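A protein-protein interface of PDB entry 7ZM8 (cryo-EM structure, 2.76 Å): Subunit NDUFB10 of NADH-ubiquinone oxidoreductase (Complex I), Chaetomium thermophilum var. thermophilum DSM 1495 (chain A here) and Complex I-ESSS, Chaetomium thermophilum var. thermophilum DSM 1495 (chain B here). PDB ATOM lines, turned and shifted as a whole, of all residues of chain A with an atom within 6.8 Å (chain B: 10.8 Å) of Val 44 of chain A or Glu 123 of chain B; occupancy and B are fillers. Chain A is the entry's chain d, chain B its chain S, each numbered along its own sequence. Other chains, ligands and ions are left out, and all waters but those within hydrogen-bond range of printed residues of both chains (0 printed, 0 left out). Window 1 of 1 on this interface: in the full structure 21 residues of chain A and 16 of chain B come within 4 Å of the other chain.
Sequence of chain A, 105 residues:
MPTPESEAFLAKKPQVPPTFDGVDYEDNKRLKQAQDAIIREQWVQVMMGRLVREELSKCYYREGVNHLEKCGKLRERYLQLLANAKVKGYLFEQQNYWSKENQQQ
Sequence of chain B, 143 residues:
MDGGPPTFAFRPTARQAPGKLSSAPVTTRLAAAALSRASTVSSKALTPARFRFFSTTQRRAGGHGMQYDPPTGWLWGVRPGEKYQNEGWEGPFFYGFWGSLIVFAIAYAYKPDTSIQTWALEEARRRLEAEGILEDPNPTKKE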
ATOM      1  N   GLU A   5      -4.583  15.326  19.276  1.00  0.00           N
ATOM      2  CA  GLU A   5      -3.846  15.929  20.376  1.00  0.00           C
ATOM      3  C   GLU A   5      -4.503  15.530  21.690  1.00  0.00           C
ATOM      4  O   GLU A   5      -5.696  15.775  21.893  1.00  0.00           O
ATOM      5  CB  GLU A   5      -3.804  17.443  20.204  1.00  0.00           C
ATOM      6  CG  GLU A   5      -2.991  18.185  21.239  1.00  0.00           C
ATOM      7  CD  GLU A   5      -2.957  19.674  20.967  1.00  0.00           C
ATOM      8  OE1 GLU A   5      -3.587  20.115  19.983  1.00  0.00           O
ATOM      9  OE2 GLU A   5      -2.294  20.403  21.728  1.00  0.00           O
ATOM     10  N   PHE A   9      -2.074  16.609  26.599  1.00  0.00           N
ATOM     11  CA  PHE A   9      -1.375  17.576  25.759  1.00  0.00           C
ATOM     12  C   PHE A   9      -2.252  18.786  25.449  1.00  0.00           C
ATOM     13  O   PHE A   9      -2.379  19.216  24.306  1.00  0.00           O
ATOM     14  CB  PHE A   9      -0.914  16.891  24.481  1.00  0.00           C
ATOM     15  CG  PHE A   9       0.272  17.535  23.836  1.00  0.00           C
ATOM     16  CD1 PHE A   9       0.155  18.750  23.179  1.00  0.00           C
ATOM     17  CD2 PHE A   9       1.497  16.920  23.868  1.00  0.00           C
ATOM     18  CE1 PHE A   9       1.231  19.341  22.593  1.00  0.00           C
ATOM     19  CE2 PHE A   9       2.576  17.510  23.272  1.00  0.00           C
ATOM     20  CZ  PHE A   9       2.440  18.723  22.636  1.00  0.00           C
ATOM     21  N   LYS A  13       0.725  22.370  27.184  1.00  0.00           N
ATOM     22  CA  LYS A  13       1.144  22.953  25.917  1.00  0.00           C
ATOM     23  C   LYS A  13       1.487  24.424  26.121  1.00  0.00           C
ATOM     24  O   LYS A  13       0.682  25.169  26.686  1.00  0.00           O
ATOM     25  CB  LYS A  13       0.052  22.792  24.865  1.00  0.00           C
ATOM     26  CG  LYS A  13       0.433  23.336  23.505  1.00  0.00           C
ATOM     27  CD  LYS A  13      -0.628  23.032  22.472  1.00  0.00           C
ATOM     28  CE  LYS A  13      -1.862  23.892  22.670  1.00  0.00           C
ATOM     29  NZ  LYS A  13      -2.865  23.684  21.589  1.00  0.00           N
ATOM     30  N   ILE A  39      12.292  25.021  26.949  1.00  0.00           N
ATOM     31  CA  ILE A  39      12.667  23.658  27.425  1.00  0.00           C
ATOM     32  C   ILE A  39      11.828  22.627  26.675  1.00  0.00           C
ATOM     33  O   ILE A  39      12.385  21.587  26.318  1.00  0.00           O
ATOM     34  CB  ILE A  39      12.512  23.550  28.960  1.00  0.00           C
ATOM     35  CG1 ILE A  39      13.472  24.479  29.704  1.00  0.00           C
ATOM     36  CG2 ILE A  39      12.648  22.113  29.433  1.00  0.00           C
ATOM     37  CD1 ILE A  39      14.927  24.160  29.490  1.00  0.00           C
ATOM     38  N   ARG A  40      10.540  22.903  26.471  1.00  0.00           N
ATOM     39  CA  ARG A  40       9.623  21.940  25.808  1.00  0.00           C
ATOM     40  C   ARG A  40      10.014  21.724  24.351  1.00  0.00           C
ATOM     41  O   ARG A  40       9.908  20.587  23.895  1.00  0.00           O
ATOM     42  CB  ARG A  40       8.164  22.317  26.041  1.00  0.00           C
ATOM     43  CG  ARG A  40       7.741  22.097  27.485  1.00  0.00           C
ATOM     44  CD  ARG A  40       6.260  22.010  27.765  1.00  0.00           C
ATOM     45  NE  ARG A  40       6.104  21.931  29.207  1.00  0.00           N
ATOM     46  CZ  ARG A  40       5.832  20.831  29.890  1.00  0.00           C
ATOM     47  NH1 ARG A  40       5.644  19.685  29.264  1.00  0.00           N
ATOM     48  NH2 ARG A  40       5.732  20.892  31.202  1.00  0.00           N
ATOM     49  N   GLU A  41      10.448  22.776  23.660  1.00  0.00           N
ATOM     50  CA  GLU A  41      10.888  22.665  22.255  1.00  0.00           C
ATOM     51  C   GLU A  41      12.143  21.803  22.168  1.00  0.00           C
ATOM     52  O   GLU A  41      12.175  20.934  21.301  1.00  0.00           O
ATOM     53  CB  GLU A  41      11.178  24.049  21.687  1.00  0.00           C
ATOM     54  CG  GLU A  41       9.961  24.729  21.095  1.00  0.00           C
ATOM     55  CD  GLU A  41       9.598  24.284  19.690  1.00  0.00           C
ATOM     56  OE1 GLU A  41      10.369  23.504  19.097  1.00  0.00           O
ATOM     57  OE2 GLU A  41       8.542  24.723  19.192  1.00  0.00           O
ATOM     58  N   GLN A  42      13.133  22.048  23.021  1.00  0.00           N
ATOM     59  CA  GLN A  42      14.417  21.307  22.995  1.00  0.00           C
ATOM     60  C   GLN A  42      14.112  19.831  23.226  1.00  0.00           C
ATOM     61  O   GLN A  42      14.724  18.998  22.559  1.00  0.00           O
ATOM     62  CB  GLN A  42      15.377  21.834  24.053  1.00  0.00           C
ATOM     63  CG  GLN A  42      15.867  23.249  23.801  1.00  0.00           C
ATOM     64  CD  GLN A  42      16.668  23.754  24.971  1.00  0.00           C
ATOM     65  OE1 GLN A  42      16.832  23.071  25.975  1.00  0.00           O
ATOM     66  NE2 GLN A  42      17.185  24.962  24.846  1.00  0.00           N
ATOM     67  N   TRP A  43      13.188  19.534  24.128  1.00  0.00           N
ATOM     68  CA  TRP A  43      12.778  18.149  24.436  1.00  0.00           C
ATOM     69  C   TRP A  43      12.015  17.473  23.291  1.00  0.00           C
ATOM     70  O   TRP A  43      12.189  16.265  23.118  1.00  0.00           O
ATOM     71  CB  TRP A  43      12.006  18.157  25.749  1.00  0.00           C
ATOM     72  CG  TRP A  43      12.873  18.011  26.957  1.00  0.00           C
ATOM     73  CD1 TRP A  43      13.263  18.995  27.813  1.00  0.00           C
ATOM     74  CD2 TRP A  43      13.465  16.798  27.447  1.00  0.00           C
ATOM     75  NE1 TRP A  43      14.048  18.478  28.803  1.00  0.00           N
ATOM     76  CE2 TRP A  43      14.195  17.135  28.604  1.00  0.00           C
ATOM     77  CE3 TRP A  43      13.446  15.466  27.028  1.00  0.00           C
ATOM     78  CZ2 TRP A  43      14.903  16.190  29.341  1.00  0.00           C
ATOM     79  CZ3 TRP A  43      14.146  14.533  27.758  1.00  0.00           C
ATOM     80  CH2 TRP A  43      14.864  14.891  28.897  1.00  0.00           C
ATOM     81  N   VAL A  44      11.162  18.197  22.579  1.00  0.00           N
ATOM     82  CA  VAL A  44      10.438  17.623  21.403  1.00  0.00           C
ATOM     83  C   VAL A  44      11.458  17.248  20.339  1.00  0.00           C
ATOM     84  O   VAL A  44      11.283  16.228  19.686  1.00  0.00           O
ATOM     85  CB  VAL A  44       9.346  18.575  20.876  1.00  0.00           C
ATOM     86  CG1 VAL A  44       8.827  18.178  19.504  1.00  0.00           C
ATOM     87  CG2 VAL A  44       8.207  18.691  21.869  1.00  0.00           C
ATOM     88  N   GLN A  45      12.482  18.065  20.197  1.00  0.00           N
ATOM     89  CA  GLN A  45      13.536  17.818  19.206  1.00  0.00           C
ATOM     90  C   GLN A  45      14.294  16.535  19.535  1.00  0.00           C
ATOM     91  O   GLN A  45      14.670  15.825  18.601  1.00  0.00           O
ATOM     92  CB  GLN A  45      14.386  19.080  19.101  1.00  0.00           C
ATOM     93  CG  GLN A  45      13.727  20.194  18.311  1.00  0.00           C
ATOM     94  CD  GLN A  45      13.239  19.704  16.972  1.00  0.00           C
ATOM     95  OE1 GLN A  45      12.061  19.795  16.653  1.00  0.00           O
ATOM     96  NE2 GLN A  45      14.147  19.163  16.180  1.00  0.00           N
ATOM     97  N   VAL A  46      14.551  16.274  20.811  1.00  0.00           N
ATOM     98  CA  VAL A  46      15.361  15.087  21.191  1.00  0.00           C
ATOM     99  C   VAL A  46      14.472  13.844  21.151  1.00  0.00           C
ATOM    100  O   VAL A  46      14.990  12.765  20.825  1.00  0.00           O
ATOM    101  CB  VAL A  46      16.118  15.289  22.519  1.00  0.00           C
ATOM    102  CG1 VAL A  46      16.857  14.038  22.960  1.00  0.00           C
ATOM    103  CG2 VAL A  46      17.068  16.472  22.456  1.00  0.00           C
ATOM    104  N   MET A  47      13.186  13.983  21.435  1.00  0.00           N
ATOM    105  CA  MET A  47      12.323  12.824  21.269  1.00  0.00           C
ATOM    106  C   MET A  47      11.987  12.573  19.813  1.00  0.00           C
ATOM    107  O   MET A  47      11.635  11.446  19.459  1.00  0.00           O
ATOM    108  CB  MET A  47      11.043  12.977  22.089  1.00  0.00           C
ATOM    109  CG  MET A  47      11.322  13.106  23.560  1.00  0.00           C
ATOM    110  SD  MET A  47      11.883  11.567  24.279  1.00  0.00           S
ATOM    111  CE  MET A  47      13.367  12.123  25.107  1.00  0.00           C
ATOM    112  N   MET A  48      12.100  13.597  18.964  1.00  0.00           N
ATOM    113  CA  MET A  48      11.988  13.386  17.529  1.00  0.00           C
ATOM    114  C   MET A  48      13.090  12.466  17.030  1.00  0.00           C
ATOM    115  O   MET A  48      12.844  11.578  16.210  1.00  0.00           O
ATOM    116  CB  MET A  48      12.048  14.724  16.797  1.00  0.00           C
ATOM    117  CG  MET A  48      10.708  15.293  16.430  1.00  0.00           C
ATOM    118  SD  MET A  48      10.830  17.004  15.936  1.00  0.00           S
ATOM    119  CE  MET A  48      11.196  16.803  14.195  1.00  0.00           C
ATOM    120  N   GLY A  49      14.317  12.679  17.510  1.00  0.00           N
ATOM    121  CA  GLY A  49      15.413  11.791  17.160  1.00  0.00           C
ATOM    122  C   GLY A  49      15.263  10.409  17.760  1.00  0.00           C
ATOM    123  O   GLY A  49      15.591   9.409  17.122  1.00  0.00           O
ATOM    124  N   LEU A  51      12.471   8.697  18.258  1.00  0.00           N
ATOM    125  CA  LEU A  51      11.497   7.987  17.395  1.00  0.00           C
ATOM    126  C   LEU A  51      12.093   7.611  16.047  1.00  0.00           C
ATOM    127  O   LEU A  51      11.814   6.502  15.591  1.00  0.00           O
ATOM    128  CB  LEU A  51      10.281   8.900  17.234  1.00  0.00           C
ATOM    129  CG  LEU A  51       9.386   9.040  18.460  1.00  0.00           C
ATOM    130  CD1 LEU A  51       8.217   9.959  18.160  1.00  0.00           C
ATOM    131  CD2 LEU A  51       8.886   7.681  18.915  1.00  0.00           C
ATOM    132  N   LEU A  81      19.396  15.323  13.277  1.00  0.00           N
ATOM    133  CA  LEU A  81      18.927  15.628  14.622  1.00  0.00           C
ATOM    134  C   LEU A  81      20.037  15.503  15.653  1.00  0.00           C
ATOM    135  O   LEU A  81      20.082  16.284  16.606  1.00  0.00           O
ATOM    136  CB  LEU A  81      17.761  14.714  14.989  1.00  0.00           C
ATOM    137  CG  LEU A  81      16.463  14.898  14.204  1.00  0.00           C
ATOM    138  CD1 LEU A  81      15.738  13.578  14.086  1.00  0.00           C
ATOM    139  CD2 LEU A  81      15.571  15.926  14.863  1.00  0.00           C
ATOM    140  N   ALA A  85      20.048  18.662  18.054  1.00  0.00           N
ATOM    141  CA  ALA A  85      19.175  18.741  19.229  1.00  0.00           C
ATOM    142  C   ALA A  85      19.908  18.268  20.464  1.00  0.00           C
ATOM    143  O   ALA A  85      20.349  17.145  20.474  1.00  0.00           O
ATOM    144  CB  ALA A  85      17.957  17.906  18.994  1.00  0.00           C
ATOM    145  N   VAL A  87      19.616  19.133  24.932  1.00  0.00           N
ATOM    146  CA  VAL A  87      18.826  19.968  25.871  1.00  0.00           C
ATOM    147  C   VAL A  87      19.857  20.886  26.515  1.00  0.00           C
ATOM    148  O   VAL A  87      20.685  20.396  27.288  1.00  0.00           O
ATOM    149  CB  VAL A  87      17.954  19.139  26.837  1.00  0.00           C
ATOM    150  CG1 VAL A  87      17.407  19.996  27.963  1.00  0.00           C
ATOM    151  CG2 VAL A  87      16.830  18.418  26.114  1.00  0.00           C
ATOM    152  N   SER B 115       5.580  13.186  33.339  1.00  0.00           N
ATOM    153  CA  SER B 115       6.983  13.253  32.846  1.00  0.00           C
ATOM    154  C   SER B 115       7.074  14.096  31.565  1.00  0.00           C
ATOM    155  O   SER B 115       6.098  14.131  30.821  1.00  0.00           O
ATOM    156  CB  SER B 115       7.494  11.865  32.614  1.00  0.00           C
ATOM    157  OG  SER B 115       8.898  11.861  32.451  1.00  0.00           O
ATOM    158  N   ILE B 116       8.207  14.749  31.319  1.00  0.00           N
ATOM    159  CA  ILE B 116       8.421  15.582  30.095  1.00  0.00           C
ATOM    160  C   ILE B 116       8.402  14.712  28.845  1.00  0.00           C
ATOM    161  O   ILE B 116       7.983  15.203  27.802  1.00  0.00           O
ATOM    162  CB  ILE B 116       9.715  16.430  30.164  1.00  0.00           C
ATOM    163  CG1 ILE B 116       9.775  17.493  29.065  1.00  0.00           C
ATOM    164  CG2 ILE B 116      10.973  15.580  30.204  1.00  0.00           C
ATOM    165  CD1 ILE B 116       8.613  18.448  29.083  1.00  0.00           C
ATOM    166  N   GLN B 117       8.804  13.456  28.957  1.00  0.00           N
ATOM    167  CA  GLN B 117       8.959  12.631  27.745  1.00  0.00           C
ATOM    168  C   GLN B 117       7.583  12.210  27.239  1.00  0.00           C
ATOM    169  O   GLN B 117       7.335  12.420  26.059  1.00  0.00           O
ATOM    170  CB  GLN B 117       9.876  11.450  28.051  1.00  0.00           C
ATOM    171  CG  GLN B 117      11.169  11.851  28.739  1.00  0.00           C
ATOM    172  CD  GLN B 117      11.153  11.473  30.197  1.00  0.00           C
ATOM    173  OE1 GLN B 117      11.167  10.300  30.555  1.00  0.00           O
ATOM    174  NE2 GLN B 117      11.118  12.473  31.057  1.00  0.00           N
ATOM    175  N   THR B 118       6.695  11.735  28.100  1.00  0.00           N
ATOM    176  CA  THR B 118       5.383  11.384  27.571  1.00  0.00           C
ATOM    177  C   THR B 118       4.743  12.556  26.848  1.00  0.00           C
ATOM    178  O   THR B 118       3.985  12.356  25.895  1.00  0.00           O
ATOM    179  CB  THR B 118       4.476  10.878  28.695  1.00  0.00           C
ATOM    180  OG1 THR B 118       3.344  10.202  28.133  1.00  0.00           O
ATOM    181  CG2 THR B 118       3.992  12.018  29.578  1.00  0.00           C
ATOM    182  N   TRP B 119       5.046  13.782  27.277  1.00  0.00           N
ATOM    183  CA  TRP B 119       4.554  14.966  26.595  1.00  0.00           C
ATOM    184  C   TRP B 119       5.336  15.234  25.320  1.00  0.00           C
ATOM    185  O   TRP B 119       4.757  15.617  24.300  1.00  0.00           O
ATOM    186  CB  TRP B 119       4.624  16.165  27.536  1.00  0.00           C
ATOM    187  CG  TRP B 119       3.998  17.399  26.972  1.00  0.00           C
ATOM    188  CD1 TRP B 119       2.744  17.848  27.206  1.00  0.00           C
ATOM    189  CD2 TRP B 119       4.614  18.357  26.105  1.00  0.00           C
ATOM    190  NE1 TRP B 119       2.525  19.012  26.530  1.00  0.00           N
ATOM    191  CE2 TRP B 119       3.660  19.349  25.845  1.00  0.00           C
ATOM    192  CE3 TRP B 119       5.879  18.471  25.527  1.00  0.00           C
ATOM    193  CZ2 TRP B 119       3.925  20.438  25.027  1.00  0.00           C
ATOM    194  CZ3 TRP B 119       6.137  19.538  24.709  1.00  0.00           C
ATOM    195  CH2 TRP B 119       5.168  20.512  24.466  1.00  0.00           C
ATOM    196  N   ALA B 120       6.648  15.042  25.365  1.00  0.00           N
ATOM    197  CA  ALA B 120       7.484  15.344  24.217  1.00  0.00           C
ATOM    198  C   ALA B 120       7.385  14.279  23.133  1.00  0.00           C
ATOM    199  O   ALA B 120       7.547  14.602  21.956  1.00  0.00           O
ATOM    200  CB  ALA B 120       8.934  15.526  24.662  1.00  0.00           C
ATOM    201  N   LEU B 121       7.140  13.015  23.497  1.00  0.00           N
ATOM    202  CA  LEU B 121       6.954  11.993  22.472  1.00  0.00           C
ATOM    203  C   LEU B 121       5.733  12.282  21.613  1.00  0.00           C
ATOM    204  O   LEU B 121       5.779  12.128  20.389  1.00  0.00           O
ATOM    205  CB  LEU B 121       6.817  10.596  23.077  1.00  0.00           C
ATOM    206  CG  LEU B 121       7.988   9.699  23.491  1.00  0.00           C
ATOM    207  CD1 LEU B 121       8.842   9.321  22.292  1.00  0.00           C
ATOM    208  CD2 LEU B 121       8.817  10.230  24.621  1.00  0.00           C
ATOM    209  N   GLU B 122       4.628  12.685  22.236  1.00  0.00           N
ATOM    210  CA  GLU B 122       3.383  12.835  21.492  1.00  0.00           C
ATOM    211  C   GLU B 122       3.458  13.999  20.512  1.00  0.00           C
ATOM    212  O   GLU B 122       2.924  13.914  19.401  1.00  0.00           O
ATOM    213  CB  GLU B 122       2.221  13.015  22.461  1.00  0.00           C
ATOM    214  CG  GLU B 122       0.885  13.212  21.788  1.00  0.00           C
ATOM    215  CD  GLU B 122      -0.125  13.839  22.705  1.00  0.00           C
ATOM    216  OE1 GLU B 122      -0.932  14.664  22.230  1.00  0.00           O
ATOM    217  OE2 GLU B 122      -0.094  13.517  23.909  1.00  0.00           O
ATOM    218  N   GLU B 123       4.103  15.098  20.909  1.00  0.00           N
ATOM    219  CA  GLU B 123       4.349  16.189  19.975  1.00  0.00           C
ATOM    220  C   GLU B 123       5.336  15.778  18.900  1.00  0.00           C
ATOM    221  O   GLU B 123       5.099  16.012  17.710  1.00  0.00           O
ATOM    222  CB  GLU B 123       4.867  17.419  20.717  1.00  0.00           C
ATOM    223  CG  GLU B 123       5.011  18.652  19.844  1.00  0.00           C
ATOM    224  CD  GLU B 123       3.823  18.860  18.913  1.00  0.00           C
ATOM    225  OE1 GLU B 123       2.676  18.929  19.398  1.00  0.00           O
ATOM    226  OE2 GLU B 123       4.037  18.944  17.687  1.00  0.00           O
ATOM    227  N   ALA B 124       6.399  15.093  19.300  1.00  0.00           N
ATOM    228  CA  ALA B 124       7.419  14.643  18.332  1.00  0.00           C
ATOM    229  C   ALA B 124       6.797  13.750  17.263  1.00  0.00           C
ATOM    230  O   ALA B 124       7.173  13.908  16.099  1.00  0.00           O
ATOM    231  CB  ALA B 124       8.510  13.934  19.067  1.00  0.00           C
ATOM    232  N   ARG B 125       5.888  12.852  17.641  1.00  0.00           N
ATOM    233  CA  ARG B 125       5.195  11.960  16.673  1.00  0.00           C
ATOM    234  C   ARG B 125       4.366  12.806  15.718  1.00  0.00           C
ATOM    235  O   ARG B 125       4.324  12.461  14.555  1.00  0.00           O
ATOM    236  CB  ARG B 125       4.294  10.955  17.387  1.00  0.00           C
ATOM    237  CG  ARG B 125       4.396   9.532  16.867  1.00  0.00           C
ATOM    238  CD  ARG B 125       3.702   8.579  17.813  1.00  0.00           C
ATOM    239  NE  ARG B 125       3.588   7.236  17.266  1.00  0.00           N
ATOM    240  CZ  ARG B 125       4.498   6.282  17.420  1.00  0.00           C
ATOM    241  NH1 ARG B 125       4.300   5.089  16.886  1.00  0.00           N
ATOM    242  NH2 ARG B 125       5.602   6.523  18.105  1.00  0.00           N
ATOM    243  N   ARG B 126       3.785  13.906  16.193  1.00  0.00           N
ATOM    244  CA  ARG B 126       2.882  14.723  15.355  1.00  0.00           C
ATOM    245  C   ARG B 126       3.720  15.567  14.404  1.00  0.00           C
ATOM    246  O   ARG B 126       3.185  15.951  13.360  1.00  0.00           O
ATOM    247  CB  ARG B 126       2.009  15.595  16.255  1.00  0.00           C
ATOM    248  CG  ARG B 126       0.555  15.156  16.313  1.00  0.00           C
ATOM    249  CD  ARG B 126      -0.293  16.237  16.949  1.00  0.00           C
ATOM    250  NE  ARG B 126       0.329  16.724  18.167  1.00  0.00           N
ATOM    251  CZ  ARG B 126       0.144  16.194  19.363  1.00  0.00           C
ATOM    252  NH1 ARG B 126       0.759  16.708  20.410  1.00  0.00           N
ATOM    253  NH2 ARG B 126      -0.646  15.150  19.509  1.00  0.00           N
ATOM    254  N   ARG B 127       4.988  15.812  14.730  1.00  0.00           N
ATOM    255  CA  ARG B 127       5.855  16.498  13.778  1.00  0.00           C
ATOM    256  C   ARG B 127       6.410  15.531  12.747  1.00  0.00           C
ATOM    257  O   ARG B 127       6.469  15.848  11.557  1.00  0.00           O
ATOM    258  CB  ARG B 127       6.991  17.202  14.511  1.00  0.00           C
ATOM    259  CG  ARG B 127       6.524  18.196  15.536  1.00  0.00           C
ATOM    260  CD  ARG B 127       7.505  19.316  15.721  1.00  0.00           C
ATOM    261  NE  ARG B 127       7.057  20.201  16.789  1.00  0.00           N
ATOM    262  CZ  ARG B 127       7.805  21.142  17.348  1.00  0.00           C
ATOM    263  NH1 ARG B 127       9.054  21.321  16.951  1.00  0.00           N
ATOM    264  NH2 ARG B 127       7.303  21.893  18.315  1.00  0.00           N
ATOM    265  N   LEU B 128       6.776  14.356  13.127  1.00  0.00           N
ATOM    266  CA  LEU B 128       7.332  13.353  12.180  1.00  0.00           C
ATOM    267  C   LEU B 128       6.200  12.741  11.364  1.00  0.00           C
ATOM    268  O   LEU B 128       6.501  12.183  10.307  1.00  0.00           O
ATOM    269  CB  LEU B 128       8.094  12.265  12.942  1.00  0.00           C
ATOM    270  CG  LEU B 128       9.273  12.724  13.796  1.00  0.00           C
ATOM    271  CD1 LEU B 128       9.698  11.619  14.746  1.00  0.00           C
ATOM    272  CD2 LEU B 128      10.442  13.151  12.929  1.00  0.00           C
ATOM    273  N   GLU B 129       4.950  12.733  11.914  1.00  0.00           N
ATOM    274  CA  GLU B 129       3.824  12.303  11.092  1.00  0.00           C
ATOM    275  C   GLU B 129       3.569  13.267   9.944  1.00  0.00           C
ATOM    276  O   GLU B 129       3.067  12.856   8.893  1.00  0.00           O
ATOM    277  CB  GLU B 129       2.574  12.134  11.948  1.00  0.00           C
ATOM    278  CG  GLU B 129       2.442  10.745  12.541  1.00  0.00           C
ATOM    279  CD  GLU B 129       1.758  10.737  13.891  1.00  0.00           C
ATOM    280  OE1 GLU B 129       1.085  11.731  14.232  1.00  0.00           O
ATOM    281  OE2 GLU B 129       1.875   9.721  14.602  1.00  0.00           O
ATOM    282  N   ALA B 130       3.959  14.527  10.135  1.00  0.00           N
ATOM    283  CA  ALA B 130       3.785  15.558   9.095  1.00  0.00           C
ATOM    284  C   ALA B 130       4.870  15.328   8.048  1.00  0.00           C
ATOM    285  O   ALA B 130       4.969  16.131   7.105  1.00  0.00           O
ATOM    286  CB  ALA B 130       3.923  16.904   9.744  1.00  0.00           C
ATOM    287  N   GLU B 131       5.647  14.264   8.218  1.00  0.00           N
ATOM    288  CA  GLU B 131       6.756  13.927   7.297  1.00  0.00           C
ATOM    289  C   GLU B 131       6.634  12.434   7.021  1.00  0.00           C
ATOM    290  O   GLU B 131       5.816  11.786   7.672  1.00  0.00           O
ATOM    291  CB  GLU B 131       8.093  14.235   7.965  1.00  0.00           C
ATOM    292  CG  GLU B 131       8.232  15.677   8.413  1.00  0.00           C
ATOM    293  CD  GLU B 131       9.137  15.890   9.613  1.00  0.00           C
ATOM    294  OE1 GLU B 131       9.437  14.901  10.308  1.00  0.00           O
ATOM    295  OE2 GLU B 131       9.541  17.045   9.849  1.00  0.00           O
ATOM    296  N   LEU B 134       7.083   9.109   9.960  1.00  0.00           N
ATOM    297  CA  LEU B 134       6.141   8.346  10.810  1.00  0.00           C
ATOM    298  C   LEU B 134       4.796   8.351  10.095  1.00  0.00           C
ATOM    299  O   LEU B 134       4.424   9.401   9.566  1.00  0.00           O
ATOM    300  CB  LEU B 134       6.065   8.979  12.207  1.00  0.00           C
ATOM    301  CG  LEU B 134       6.719   8.202  13.346  1.00  0.00           C
ATOM    302  CD1 LEU B 134       8.117   7.745  12.973  1.00  0.00           C
ATOM    303  CD2 LEU B 134       6.775   9.061  14.587  1.00  0.00           C
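The side-chain carboxylate (OE2) of Glu 41 of chain A lies within salt-bridge range of the guanidinium group (NH2) of Arg 127 of chain B (3.2 Å).
NH1 of Arg 127 of chain B lies within hydrogen-bond range of OE1 of Gln 45 of chain A (3.4 Å).
OE1 of Gln 45 of chain A sits close to SD of Met 48 of chain A, 3.1 Å away.
OE1 of Glu 123 of chain B lies within salt-bridge range of NH1 of Arg 126 of chain B.
The side-chain amino group of Lys 13 of chain A is in salt-bridge range of the side-chain carboxylate of Glu 5 of chain A, at 3.3 Å.
The side-chain carboxylate (OE1) of Glu 122 of chain B lies within salt-bridge range of the guanidinium group (NH2) of Arg 126 of chain B, at 2.8 Å.
The side-chain carboxylate of Glu 123 of chain B lies within salt-bridge range of the guanidinium group of Arg 127 of chain B, 3.4 Å away.
N of Leu 134 of chain B lies within hydrogen-bond range of O of Leu 128 of chain B, at 3.1 Å.
Glu 122 of chain B touches Glu 5 of chain A (OE1 to CA, 3.7 Å).
Glu 123 of chain B touches Phe 9 of chain A (OE1 to CZ, 3.3 Å).
Trp 119 of chain B touches Lys 13 of chain A.
CD2 of Trp 119 of chain B touches NH1 of Arg 40 of chain A, 3.6 Å away.
Ala 120 of chain B touches Met 47 of chain A.
Met 48 of chain A touches Ala 124 of chain B (N to CB, 3.6 Å).
Leu 51 of chain A touches Leu 121 of chain B.
Leu 51 of chain A touches Arg 125 of chain B (CD2 to NH2, 3.6 Å).
CB of Leu 51 of chain A touches CD1 of Leu 128 of chain B (3.7 Å).
Leu 51 of chain A touches Leu 134 of chain B (CD1 to CD2, 3.96 Å).
Printed residues of chain B within 4 Å of Val 44 of chain A: Trp 119, Glu 123, Ala 124 and Arg 127.
Of the printed residues of chain A, Glu 123 of chain B touches Phe 9 (3.3 Å) and Val 44 (3.8 Å).
Of chain B, only Arg 127 comes within 4 Å of Gln 45 of chain A.
Met 48 of chain A touches just these residues of chain B: Ala 124 (3.6 Å) and Leu 128 (3.5 Å).
Of the printed residues of chain B, Met 47 of chain A touches Ala 120 (3.6 Å), Leu 121 (3.4 Å) and Ala 124 (3.8 Å).
Printed residues of chain A within 4 Å of Leu 134 of chain B: Leu 51.
Glu 129 of chain B touches none of the printed residues of chain A.
The nearest residue of chain B that does not touch Val 44 of chain A is Ala 120 of chain B (4.1 Å).
The nearest printed residue of chain B that does not touch Trp 43 of chain A is Gln 117 of chain B (4.1 Å).
Along chain A the printed residues that touch a printed residue of chain B span positions 5 to 51.
Among the printed residues, Asp or Glu carboxylates within 4 Å of a Lys or Arg side-chain nitrogen of the other chain: Glu 41 of chain A with Arg 127 of chain B.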
